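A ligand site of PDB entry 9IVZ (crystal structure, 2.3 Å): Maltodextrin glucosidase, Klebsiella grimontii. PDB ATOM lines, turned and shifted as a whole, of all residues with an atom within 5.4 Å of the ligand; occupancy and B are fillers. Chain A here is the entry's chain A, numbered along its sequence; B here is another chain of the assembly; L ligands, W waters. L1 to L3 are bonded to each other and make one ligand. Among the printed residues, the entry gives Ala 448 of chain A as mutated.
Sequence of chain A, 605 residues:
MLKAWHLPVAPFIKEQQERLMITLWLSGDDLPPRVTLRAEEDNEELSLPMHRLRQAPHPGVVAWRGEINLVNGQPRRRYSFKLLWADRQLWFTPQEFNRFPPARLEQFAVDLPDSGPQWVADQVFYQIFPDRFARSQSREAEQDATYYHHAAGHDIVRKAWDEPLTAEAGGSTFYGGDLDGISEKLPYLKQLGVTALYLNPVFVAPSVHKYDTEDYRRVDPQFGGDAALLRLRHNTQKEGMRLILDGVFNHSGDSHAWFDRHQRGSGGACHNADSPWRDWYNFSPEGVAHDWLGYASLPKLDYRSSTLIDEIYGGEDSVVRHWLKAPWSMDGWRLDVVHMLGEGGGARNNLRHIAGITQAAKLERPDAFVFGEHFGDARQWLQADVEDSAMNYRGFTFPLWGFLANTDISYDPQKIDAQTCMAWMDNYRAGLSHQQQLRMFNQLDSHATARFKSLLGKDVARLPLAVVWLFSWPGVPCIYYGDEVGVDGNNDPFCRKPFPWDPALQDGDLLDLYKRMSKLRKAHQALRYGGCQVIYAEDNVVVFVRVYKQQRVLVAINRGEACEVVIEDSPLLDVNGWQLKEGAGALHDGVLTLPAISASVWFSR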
ATOM      1  N   GLY A 170       2.451  18.861 -16.632  1.00  0.00           N
ATOM      2  CA  GLY A 170       1.330  19.785 -16.734  1.00  0.00           C
ATOM      3  C   GLY A 170      -0.028  19.119 -16.889  1.00  0.00           C
ATOM      4  O   GLY A 170      -1.046  19.695 -16.516  1.00  0.00           O
ATOM      5  N   GLY A 171      -0.067  17.911 -17.427  1.00  0.00           N
ATOM      6  CA  GLY A 171      -1.307  17.194 -17.602  1.00  0.00           C
ATOM      7  C   GLY A 171      -1.599  16.181 -16.538  1.00  0.00           C
ATOM      8  O   GLY A 171      -2.657  15.532 -16.594  1.00  0.00           O
ATOM      9  N   VAL A 208      -5.386  15.384 -15.927  1.00  0.00           N
ATOM     10  CA  VAL A 208      -6.075  16.350 -15.067  1.00  0.00           C
ATOM     11  C   VAL A 208      -7.092  17.149 -15.865  1.00  0.00           C
ATOM     12  O   VAL A 208      -8.122  17.563 -15.316  1.00  0.00           O
ATOM     13  CB  VAL A 208      -5.055  17.270 -14.379  1.00  0.00           C
ATOM     14  CG1 VAL A 208      -4.292  18.114 -15.417  1.00  0.00           C
ATOM     15  CG2 VAL A 208      -5.740  18.170 -13.362  1.00  0.00           C
ATOM     16  N   HIS A 209      -6.856  17.386 -17.154  1.00  0.00           N
ATOM     17  CA  HIS A 209      -7.799  18.149 -17.963  1.00  0.00           C
ATOM     18  C   HIS A 209      -8.906  17.279 -18.536  1.00  0.00           C
ATOM     19  O   HIS A 209     -10.016  17.769 -18.770  1.00  0.00           O
ATOM     20  CB  HIS A 209      -7.039  18.864 -19.071  1.00  0.00           C
ATOM     21  CG  HIS A 209      -6.189  17.952 -19.899  1.00  0.00           C
ATOM     22  ND1 HIS A 209      -6.724  17.080 -20.829  1.00  0.00           N
ATOM     23  CD2 HIS A 209      -4.861  17.729 -19.891  1.00  0.00           C
ATOM     24  CE1 HIS A 209      -5.750  16.372 -21.363  1.00  0.00           C
ATOM     25  NE2 HIS A 209      -4.605  16.749 -20.824  1.00  0.00           N
ATOM     26  N   TYR A 211      -9.429  15.753 -21.457  1.00  0.00           N
ATOM     27  CA  TYR A 211      -9.807  15.661 -22.872  1.00  0.00           C
ATOM     28  C   TYR A 211      -9.392  14.327 -23.471  1.00  0.00           C
ATOM     29  O   TYR A 211      -9.722  14.043 -24.628  1.00  0.00           O
ATOM     30  CB  TYR A 211      -9.210  16.822 -23.674  1.00  0.00           C
ATOM     31  CG  TYR A 211      -9.896  18.143 -23.401  1.00  0.00           C
ATOM     32  CD1 TYR A 211     -11.135  18.435 -23.980  1.00  0.00           C
ATOM     33  CD2 TYR A 211      -9.331  19.082 -22.554  1.00  0.00           C
ATOM     34  CE1 TYR A 211     -11.789  19.646 -23.719  1.00  0.00           C
ATOM     35  CE2 TYR A 211      -9.983  20.284 -22.267  1.00  0.00           C
ATOM     36  CZ  TYR A 211     -11.202  20.557 -22.854  1.00  0.00           C
ATOM     37  OH  TYR A 211     -11.829  21.757 -22.554  1.00  0.00           O
ATOM     38  N   VAL A 248     -16.323  16.119 -25.925  1.00  0.00           N
ATOM     39  CA  VAL A 248     -15.041  15.836 -26.579  1.00  0.00           C
ATOM     40  C   VAL A 248     -15.214  14.679 -27.564  1.00  0.00           C
ATOM     41  O   VAL A 248     -14.908  13.535 -27.247  1.00  0.00           O
ATOM     42  CB  VAL A 248     -13.951  15.530 -25.542  1.00  0.00           C
ATOM     43  CG1 VAL A 248     -12.551  15.602 -26.185  1.00  0.00           C
ATOM     44  CG2 VAL A 248     -14.062  16.504 -24.363  1.00  0.00           C
ATOM     45  N   HIS A 251     -12.123  13.127 -30.815  1.00  0.00           N
ATOM     46  CA  HIS A 251     -11.090  12.173 -30.484  1.00  0.00           C
ATOM     47  C   HIS A 251     -11.411  11.593 -29.113  1.00  0.00           C
ATOM     48  O   HIS A 251     -12.075  12.240 -28.306  1.00  0.00           O
ATOM     49  CB  HIS A 251      -9.719  12.852 -30.476  1.00  0.00           C
ATOM     50  CG  HIS A 251      -9.598  13.887 -29.404  1.00  0.00           C
ATOM     51  ND1 HIS A 251      -9.726  15.237 -29.641  1.00  0.00           N
ATOM     52  CD2 HIS A 251      -9.416  13.763 -28.064  1.00  0.00           C
ATOM     53  CE1 HIS A 251      -9.592  15.903 -28.511  1.00  0.00           C
ATOM     54  NE2 HIS A 251      -9.410  15.026 -27.534  1.00  0.00           N
ATOM     55  N   TRP A 292      -2.756  11.314 -33.675  1.00  0.00           N
ATOM     56  CA  TRP A 292      -3.501  12.479 -34.159  1.00  0.00           C
ATOM     57  C   TRP A 292      -2.682  13.722 -33.850  1.00  0.00           C
ATOM     58  O   TRP A 292      -2.329  13.966 -32.695  1.00  0.00           O
ATOM     59  CB  TRP A 292      -4.894  12.591 -33.539  1.00  0.00           C
ATOM     60  CG  TRP A 292      -5.596  13.835 -34.034  1.00  0.00           C
ATOM     61  CD1 TRP A 292      -5.829  14.177 -35.342  1.00  0.00           C
ATOM     62  CD2 TRP A 292      -6.140  14.904 -33.244  1.00  0.00           C
ATOM     63  NE1 TRP A 292      -6.473  15.398 -35.412  1.00  0.00           N
ATOM     64  CE2 TRP A 292      -6.682  15.858 -34.145  1.00  0.00           C
ATOM     65  CE3 TRP A 292      -6.235  15.157 -31.866  1.00  0.00           C
ATOM     66  CZ2 TRP A 292      -7.299  17.034 -33.696  1.00  0.00           C
ATOM     67  CZ3 TRP A 292      -6.842  16.312 -31.441  1.00  0.00           C
ATOM     68  CH2 TRP A 292      -7.372  17.240 -32.352  1.00  0.00           C
ATOM     69  N   LEU A 293      -2.419  14.513 -34.882  1.00  0.00           N
ATOM     70  CA  LEU A 293      -1.472  15.625 -34.774  1.00  0.00           C
ATOM     71  C   LEU A 293      -0.223  15.101 -34.071  1.00  0.00           C
ATOM     72  O   LEU A 293       0.370  14.119 -34.515  1.00  0.00           O
ATOM     73  CB  LEU A 293      -2.084  16.818 -34.040  1.00  0.00           C
ATOM     74  CG  LEU A 293      -3.328  17.425 -34.728  1.00  0.00           C
ATOM     75  CD1 LEU A 293      -3.653  18.813 -34.189  1.00  0.00           C
ATOM     76  CD2 LEU A 293      -3.225  17.450 -36.245  1.00  0.00           C
ATOM     77  N   TYR A 295      -0.274  13.784 -31.027  1.00  0.00           N
ATOM     78  CA  TYR A 295      -0.731  13.124 -29.806  1.00  0.00           C
ATOM     79  C   TYR A 295      -0.924  11.637 -30.013  1.00  0.00           C
ATOM     80  O   TYR A 295      -1.806  11.213 -30.776  1.00  0.00           O
ATOM     81  CB  TYR A 295      -2.047  13.743 -29.327  1.00  0.00           C
ATOM     82  CG  TYR A 295      -1.976  15.218 -29.086  1.00  0.00           C
ATOM     83  CD1 TYR A 295      -1.323  15.716 -27.963  1.00  0.00           C
ATOM     84  CD2 TYR A 295      -2.580  16.112 -29.967  1.00  0.00           C
ATOM     85  CE1 TYR A 295      -1.264  17.079 -27.709  1.00  0.00           C
ATOM     86  CE2 TYR A 295      -2.522  17.480 -29.727  1.00  0.00           C
ATOM     87  CZ  TYR A 295      -1.858  17.963 -28.595  1.00  0.00           C
ATOM     88  OH  TYR A 295      -1.790  19.312 -28.332  1.00  0.00           O
ATOM     89  N   SER A 297      -1.836  10.258 -27.221  1.00  0.00           N
ATOM     90  CA  SER A 297      -2.875  10.100 -26.204  1.00  0.00           C
ATOM     91  C   SER A 297      -4.280  10.377 -26.723  1.00  0.00           C
ATOM     92  O   SER A 297      -5.242   9.963 -26.071  1.00  0.00           O
ATOM     93  CB  SER A 297      -2.589  11.003 -25.003  1.00  0.00           C
ATOM     94  OG  SER A 297      -2.484  12.353 -25.400  1.00  0.00           O
ATOM     95  N   LEU A 298      -4.431  11.051 -27.861  1.00  0.00           N
ATOM     96  CA  LEU A 298      -5.727  11.557 -28.318  1.00  0.00           C
ATOM     97  C   LEU A 298      -6.080  11.063 -29.718  1.00  0.00           C
ATOM     98  O   LEU A 298      -6.283  11.868 -30.629  1.00  0.00           O
ATOM     99  CB  LEU A 298      -5.757  13.082 -28.278  1.00  0.00           C
ATOM    100  CG  LEU A 298      -5.337  13.812 -26.999  1.00  0.00           C
ATOM    101  CD1 LEU A 298      -5.186  15.289 -27.224  1.00  0.00           C
ATOM    102  CD2 LEU A 298      -6.348  13.549 -25.895  1.00  0.00           C
ATOM    103  N   ASP A 336     -15.772  20.382 -28.066  1.00  0.00           N
ATOM    104  CA  ASP A 336     -14.325  20.519 -28.174  1.00  0.00           C
ATOM    105  C   ASP A 336     -13.863  20.154 -29.581  1.00  0.00           C
ATOM    106  O   ASP A 336     -14.416  19.236 -30.187  1.00  0.00           O
ATOM    107  CB  ASP A 336     -13.644  19.618 -27.149  1.00  0.00           C
ATOM    108  CG  ASP A 336     -12.126  19.729 -27.181  1.00  0.00           C
ATOM    109  OD1 ASP A 336     -11.612  20.843 -26.990  1.00  0.00           O
ATOM    110  OD2 ASP A 336     -11.449  18.706 -27.388  1.00  0.00           O
ATOM    111  N   VAL A 337     -12.856  20.872 -30.085  1.00  0.00           N
ATOM    112  CA  VAL A 337     -12.308  20.686 -31.439  1.00  0.00           C
ATOM    113  C   VAL A 337     -13.434  20.531 -32.441  1.00  0.00           C
ATOM    114  O   VAL A 337     -13.473  19.557 -33.201  1.00  0.00           O
ATOM    115  CB  VAL A 337     -11.349  19.467 -31.489  1.00  0.00           C
ATOM    116  CG1 VAL A 337     -10.502  19.504 -32.764  1.00  0.00           C
ATOM    117  CG2 VAL A 337     -10.457  19.407 -30.271  1.00  0.00           C
ATOM    118  N   HIS A 339     -14.184  22.090 -35.121  1.00  0.00           N
ATOM    119  CA  HIS A 339     -13.848  22.367 -36.507  1.00  0.00           C
ATOM    120  C   HIS A 339     -13.056  21.245 -37.182  1.00  0.00           C
ATOM    121  O   HIS A 339     -12.896  21.273 -38.407  1.00  0.00           O
ATOM    122  CB  HIS A 339     -13.050  23.667 -36.570  1.00  0.00           C
ATOM    123  CG  HIS A 339     -11.721  23.589 -35.865  1.00  0.00           C
ATOM    124  ND1 HIS A 339     -11.588  23.105 -34.580  1.00  0.00           N
ATOM    125  CD2 HIS A 339     -10.471  23.915 -36.282  1.00  0.00           C
ATOM    126  CE1 HIS A 339     -10.315  23.150 -34.234  1.00  0.00           C
ATOM    127  NE2 HIS A 339      -9.619  23.632 -35.243  1.00  0.00           N
ATOM    128  N   MET A 340     -12.538  20.273 -36.438  1.00  0.00           N
ATOM    129  CA  MET A 340     -11.708  19.240 -37.037  1.00  0.00           C
ATOM    130  C   MET A 340     -12.355  17.863 -37.029  1.00  0.00           C
ATOM    131  O   MET A 340     -11.882  16.973 -37.740  1.00  0.00           O
ATOM    132  CB  MET A 340     -10.351  19.163 -36.341  1.00  0.00           C
ATOM    133  CG  MET A 340      -9.606  20.489 -36.344  1.00  0.00           C
ATOM    134  SD  MET A 340      -7.964  20.420 -35.612  1.00  0.00           S
ATOM    135  CE  MET A 340      -7.054  19.617 -36.933  1.00  0.00           C
ATOM    136  N   GLU A 373     -15.931  25.274 -29.842  1.00  0.00           N
ATOM    137  CA  GLU A 373     -14.726  26.068 -29.636  1.00  0.00           C
ATOM    138  C   GLU A 373     -14.121  26.402 -30.997  1.00  0.00           C
ATOM    139  O   GLU A 373     -13.616  25.517 -31.693  1.00  0.00           O
ATOM    140  CB  GLU A 373     -13.722  25.312 -28.776  1.00  0.00           C
ATOM    141  CG  GLU A 373     -12.392  26.023 -28.670  1.00  0.00           C
ATOM    142  CD  GLU A 373     -11.293  25.156 -28.054  1.00  0.00           C
ATOM    143  OE1 GLU A 373     -10.897  24.127 -28.675  1.00  0.00           O
ATOM    144  OE2 GLU A 373     -10.835  25.523 -26.936  1.00  0.00           O
ATOM    145  N   PHE A 375     -11.279  28.763 -32.262  1.00  0.00           N
ATOM    146  CA  PHE A 375     -10.183  29.735 -32.353  1.00  0.00           C
ATOM    147  C   PHE A 375     -10.208  30.463 -33.683  1.00  0.00           C
ATOM    148  O   PHE A 375      -9.761  31.614 -33.777  1.00  0.00           O
ATOM    149  CB  PHE A 375      -8.842  29.038 -32.144  1.00  0.00           C
ATOM    150  CG  PHE A 375      -8.456  28.881 -30.694  1.00  0.00           C
ATOM    151  CD1 PHE A 375      -9.159  28.002 -29.869  1.00  0.00           C
ATOM    152  CD2 PHE A 375      -7.434  29.627 -30.153  1.00  0.00           C
ATOM    153  CE1 PHE A 375      -8.826  27.857 -28.517  1.00  0.00           C
ATOM    154  CE2 PHE A 375      -7.087  29.495 -28.797  1.00  0.00           C
ATOM    155  CZ  PHE A 375      -7.793  28.607 -27.983  1.00  0.00           C
ATOM    156  N   HIS A 447      -9.043  28.044 -20.639  1.00  0.00           N
ATOM    157  CA  HIS A 447      -8.069  27.019 -20.308  1.00  0.00           C
ATOM    158  C   HIS A 447      -7.048  26.778 -21.412  1.00  0.00           C
ATOM    159  O   HIS A 447      -6.067  26.067 -21.183  1.00  0.00           O
ATOM    160  CB  HIS A 447      -8.788  25.715 -20.011  1.00  0.00           C
ATOM    161  CG  HIS A 447      -9.511  25.174 -21.191  1.00  0.00           C
ATOM    162  ND1 HIS A 447     -10.619  25.796 -21.724  1.00  0.00           N
ATOM    163  CD2 HIS A 447      -9.259  24.097 -21.986  1.00  0.00           C
ATOM    164  CE1 HIS A 447     -11.043  25.115 -22.787  1.00  0.00           C
ATOM    165  NE2 HIS A 447     -10.232  24.085 -22.961  1.00  0.00           N
ATOM    166  N   ALA A 448      -7.283  27.322 -22.615  1.00  0.00           N
ATOM    167  CA  ALA A 448      -6.436  27.111 -23.779  1.00  0.00           C
ATOM    168  C   ALA A 448      -5.700  28.373 -24.206  1.00  0.00           C
ATOM    169  O   ALA A 448      -5.078  28.389 -25.278  1.00  0.00           O
ATOM    170  CB  ALA A 448      -7.264  26.560 -24.940  1.00  0.00           C
ATOM    171  N   ASP A 492      -1.351  27.606 -20.886  1.00  0.00           N
ATOM    172  CA  ASP A 492      -1.364  26.187 -20.551  1.00  0.00           C
ATOM    173  C   ASP A 492       0.060  25.651 -20.423  1.00  0.00           C
ATOM    174  O   ASP A 492       0.804  25.627 -21.413  1.00  0.00           O
ATOM    175  CB  ASP A 492      -2.150  25.460 -21.645  1.00  0.00           C
ATOM    176  CG  ASP A 492      -2.326  23.997 -21.368  1.00  0.00           C
ATOM    177  OD1 ASP A 492      -2.112  23.570 -20.218  1.00  0.00           O
ATOM    178  OD2 ASP A 492      -2.691  23.262 -22.319  1.00  0.00           O
ATOM    179  N   PRO A 493       0.466  25.179 -19.235  1.00  0.00           N
ATOM    180  CA  PRO A 493      -0.321  24.895 -18.025  1.00  0.00           C
ATOM    181  C   PRO A 493      -0.635  26.074 -17.082  1.00  0.00           C
ATOM    182  O   PRO A 493      -1.489  25.904 -16.210  1.00  0.00           O
ATOM    183  CB  PRO A 493       0.558  23.877 -17.307  1.00  0.00           C
ATOM    184  CG  PRO A 493       1.935  24.336 -17.615  1.00  0.00           C
ATOM    185  CD  PRO A 493       1.869  24.763 -19.070  1.00  0.00           C
ATOM    186  N   ARG A 496      -4.159  27.686 -15.600  1.00  0.00           N
ATOM    187  CA  ARG A 496      -5.041  26.845 -14.795  1.00  0.00           C
ATOM    188  C   ARG A 496      -4.613  26.852 -13.332  1.00  0.00           C
ATOM    189  O   ARG A 496      -4.559  25.802 -12.683  1.00  0.00           O
ATOM    190  CB  ARG A 496      -5.063  25.425 -15.359  1.00  0.00           C
ATOM    191  CG  ARG A 496      -5.433  25.386 -16.830  1.00  0.00           C
ATOM    192  CD  ARG A 496      -4.995  24.113 -17.515  1.00  0.00           C
ATOM    193  NE  ARG A 496      -5.259  24.234 -18.941  1.00  0.00           N
ATOM    194  CZ  ARG A 496      -5.318  23.217 -19.792  1.00  0.00           C
ATOM    195  NH1 ARG A 496      -5.091  21.969 -19.394  1.00  0.00           N
ATOM    196  NH2 ARG A 496      -5.623  23.460 -21.064  1.00  0.00           N
ATOM    197  N   GLU B  44      -7.914  23.899 -39.115  1.00  0.00           N
ATOM    198  CA  GLU B  44      -7.077  24.491 -38.074  1.00  0.00           C
ATOM    199  C   GLU B  44      -6.127  25.509 -38.698  1.00  0.00           C
ATOM    200  O   GLU B  44      -5.497  25.241 -39.725  1.00  0.00           O
ATOM    201  CB  GLU B  44      -6.293  23.420 -37.332  1.00  0.00           C
ATOM    202  CG  GLU B  44      -5.235  23.955 -36.373  1.00  0.00           C
ATOM    203  CD  GLU B  44      -5.821  24.459 -35.065  1.00  0.00           C
ATOM    204  OE1 GLU B  44      -7.015  24.814 -35.041  1.00  0.00           O
ATOM    205  OE2 GLU B  44      -5.075  24.505 -34.063  1.00  0.00           O
HETATM  206  C1  LIG L   1      -6.252  25.643 -30.989  1.00  0.00           C
HETATM  207  C2  LIG L   1      -7.163  24.531 -31.492  1.00  0.00           C
HETATM  208  C3  LIG L   1      -7.935  23.846 -30.387  1.00  0.00           C
HETATM  209  C4  LIG L   1      -7.308  23.925 -28.994  1.00  0.00           C
HETATM  210  C5  LIG L   1      -5.962  24.676 -28.821  1.00  0.00           C
HETATM  211  C6  LIG L   1      -5.029  24.056 -27.837  1.00  0.00           C
HETATM  212  O1  LIG L   1      -5.580  26.281 -32.075  1.00  0.00           O
HETATM  213  O2  LIG L   1      -8.054  25.097 -32.453  1.00  0.00           O
HETATM  214  O3  LIG L   1      -8.335  22.518 -30.808  1.00  0.00           O
HETATM  215  O4  LIG L   1      -7.512  22.863 -27.999  1.00  0.00           O
HETATM  216  O5  LIG L   1      -5.262  25.043 -30.085  1.00  0.00           O
HETATM  217  O6  LIG L   1      -3.920  23.538 -28.491  1.00  0.00           O
HETATM  218  C1  LG2 L   2      -7.377  21.482 -28.151  1.00  0.00           C
HETATM  219  C2  LG2 L   2      -8.153  20.920 -26.977  1.00  0.00           C
HETATM  220  C3  LG2 L   2      -7.852  19.529 -26.585  1.00  0.00           C
HETATM  221  C4  LG2 L   2      -6.405  19.190 -26.590  1.00  0.00           C
HETATM  222  C5  LG2 L   2      -5.662  19.727 -27.809  1.00  0.00           C
HETATM  223  C6  LG2 L   2      -5.947  18.943 -29.109  1.00  0.00           C
HETATM  224  O1  LG2 L   2      -7.936  21.762 -25.772  1.00  0.00           O
HETATM  225  O2  LG2 L   2      -8.625  18.627 -27.443  1.00  0.00           O
HETATM  226  O3  LG2 L   2      -5.749  19.798 -25.380  1.00  0.00           O
HETATM  227  O4  LG2 L   2      -5.937  21.144 -28.080  1.00  0.00           O
HETATM  228  O5  LG2 L   2      -5.192  19.554 -30.158  1.00  0.00           O
HETATM  229  O1  LG3 L   3      -4.976  17.843 -24.202  1.00  0.00           O
HETATM  230  C1  LG3 L   3      -5.420  19.920 -22.999  1.00  0.00           C
HETATM  231  C2  LG3 L   3      -3.984  20.346 -23.052  1.00  0.00           C
HETATM  232  C3  LG3 L   3      -0.951  19.205 -20.620  1.00  0.00           C
HETATM  233  C4  LG3 L   3       2.879  18.742 -22.587  1.00  0.00           C
HETATM  234  C5  LG3 L   3       1.462  19.275 -22.262  1.00  0.00           C
HETATM  235  C6  LG3 L   3       0.250  18.263 -22.632  1.00  0.00           C
HETATM  236  C7  LG3 L   3      -1.077  18.550 -22.185  1.00  0.00           C
HETATM  237  C8  LG3 L   3      -2.992  19.460 -23.781  1.00  0.00           C
HETATM  238  C9  LG3 L   3      -3.552  18.175 -24.523  1.00  0.00           C
HETATM  239  C10 LG3 L   3      -2.769  16.904 -24.497  1.00  0.00           C
HETATM  240  C11 LG3 L   3      -5.836  19.034 -24.177  1.00  0.00           C
HETATM  241  C12 LG3 L   3      -0.357  20.367 -20.689  1.00  0.00           C
HETATM  242  C13 LG3 L   3       1.296  20.135 -21.114  1.00  0.00           C
HETATM  243  N1  LG3 L   3      -1.598  19.522 -23.127  1.00  0.00           N
HETATM  244  O2  LG3 L   3       3.831  19.810 -22.556  1.00  0.00           O
HETATM  245  O3  LG3 L   3      -6.198  21.106 -23.057  1.00  0.00           O
HETATM  246  O4  LG3 L   3      -3.528  20.744 -21.725  1.00  0.00           O
HETATM  247  O5  LG3 L   3      -2.280  19.290 -20.052  1.00  0.00           O
HETATM  248  O6  LG3 L   3      -0.389  21.109 -19.444  1.00  0.00           O
HETATM  249  O7  LG3 L   3       1.855  21.383 -21.339  1.00  0.00           O
HETATM  250  O   HOH W   1     -10.390  22.713 -25.614  1.00  0.00           O
HETATM  251  O   HOH W   2      -0.560  20.046 -25.527  1.00  0.00           O
HETATM  252  O   HOH W   3      -4.248  23.925 -24.658  1.00  0.00           O
HETATM  253  O   HOH W   4       6.154  21.341 -22.931  1.00  0.00           O
HETATM  254  O   HOH W   5     -10.846  25.838 -32.374  1.00  0.00           O
HETATM  255  O   HOH W   6      -6.819  20.867 -32.039  1.00  0.00           O
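CA of Gly 171 touches O5 of LG3 L3, 3.4 Å away.
CD2 of His 209 touches O5 of LG3 L3 (3.0 Å).
CD2 of Tyr 211 touches O3 of LG3 L3, 3.8 Å away.
CE1 of His 251 touches O2 of LG2 L2, at 3.1 Å.
CZ3 of Trp 292 touches C6 of LG2 L2 (3.6 Å).
CE2 of Tyr 295 touches O5 of LG2 L2 (3.4 Å).
CD1 of Leu 298 touches O1 of LG3 L3 (3.96 Å).
CG2 of Val 337 touches O2 of LG2 L2, at 3.5 Å.
CE1 of His 339 touches O2 of LIG L1, 3.5 Å away.
OE1 of Glu 373 touches C3 of LIG L1, 3.4 Å away.
CD1 of Phe 375 touches C1 of LIG L1, at 3.9 Å.
CB of Pro 493 touches O6 of LG3 L3 (3.6 Å).
Of the 24 residues printed, 17 come within 4 Å of the ligand.
Water W6 bridges an oxygen (O3) of LIG L1 (2.6 Å) and the side-chain sulfur of Met 340 (3.8 Å).
Water W1 lies within hydrogen-bond range of the side-chain carboxylate (OD1) of Asp 336 (2.6 Å), an oxygen (O1) of LG2 L2 (2.6 Å), a ring nitrogen (NE2) of His 447 (3.0 Å) and the side-chain carboxylate (OE2) of Glu 373 (3.1 Å).
Water W2 bridges N1 of LG3 L3 and OH of Tyr 295.
Water W5 lies within hydrogen-bond range of O of Glu 373, O2 of LIG L1 and N of Phe 375.
A ring nitrogen (NE2) of His 251 lies within hydrogen-bond range of the backbone carbonyl oxygen of Tyr 211, at 3.1 Å.
N of Tyr 211 lies within hydrogen-bond range of ND1 of His 209, 3.1 Å away.
NH2 of Arg 496 sits at hydrogen-bond distance from O of His 447 (2.6 Å).
The guanidinium group of Arg 496 is in salt-bridge range of the side-chain carboxylate of Asp 492 (3.2 Å).
NE2 of His 339 lies close to SD of Met 340, 3.6 Å away.
The side-chain carboxylate (OE1) of Glu 44 of chain B sits at hydrogen-bond distance from a ring nitrogen (NE2) of His 339 (2.9 Å).
A ring nitrogen (NE2) of His 447 is in hydrogen-bond range of the side-chain hydroxyl (OH) of Tyr 211.
N of Val 208 lies within hydrogen-bond range of O of Gly 171, 2.8 Å away.
OE2 of Glu 44 of chain B lies within hydrogen-bond range of O1 of LIG L1 (2.7 Å).
The side-chain carboxylate (OD2) of Asp 492 lies within salt-bridge range of a nitrogen (N1) of LG3 L3.
The guanidinium group (NH1) of Arg 496 lies within hydrogen-bond range of an oxygen (O4) of LG3 L3, 3.1 Å away.
An oxygen (O2) of LG2 L2 sits at hydrogen-bond distance from the side-chain carboxylate of Asp 336 (2.8 Å).
An oxygen (O6) of LG3 L3 sits close to the backbone carbonyl oxygen of Gly 170, 3.3 Å away.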
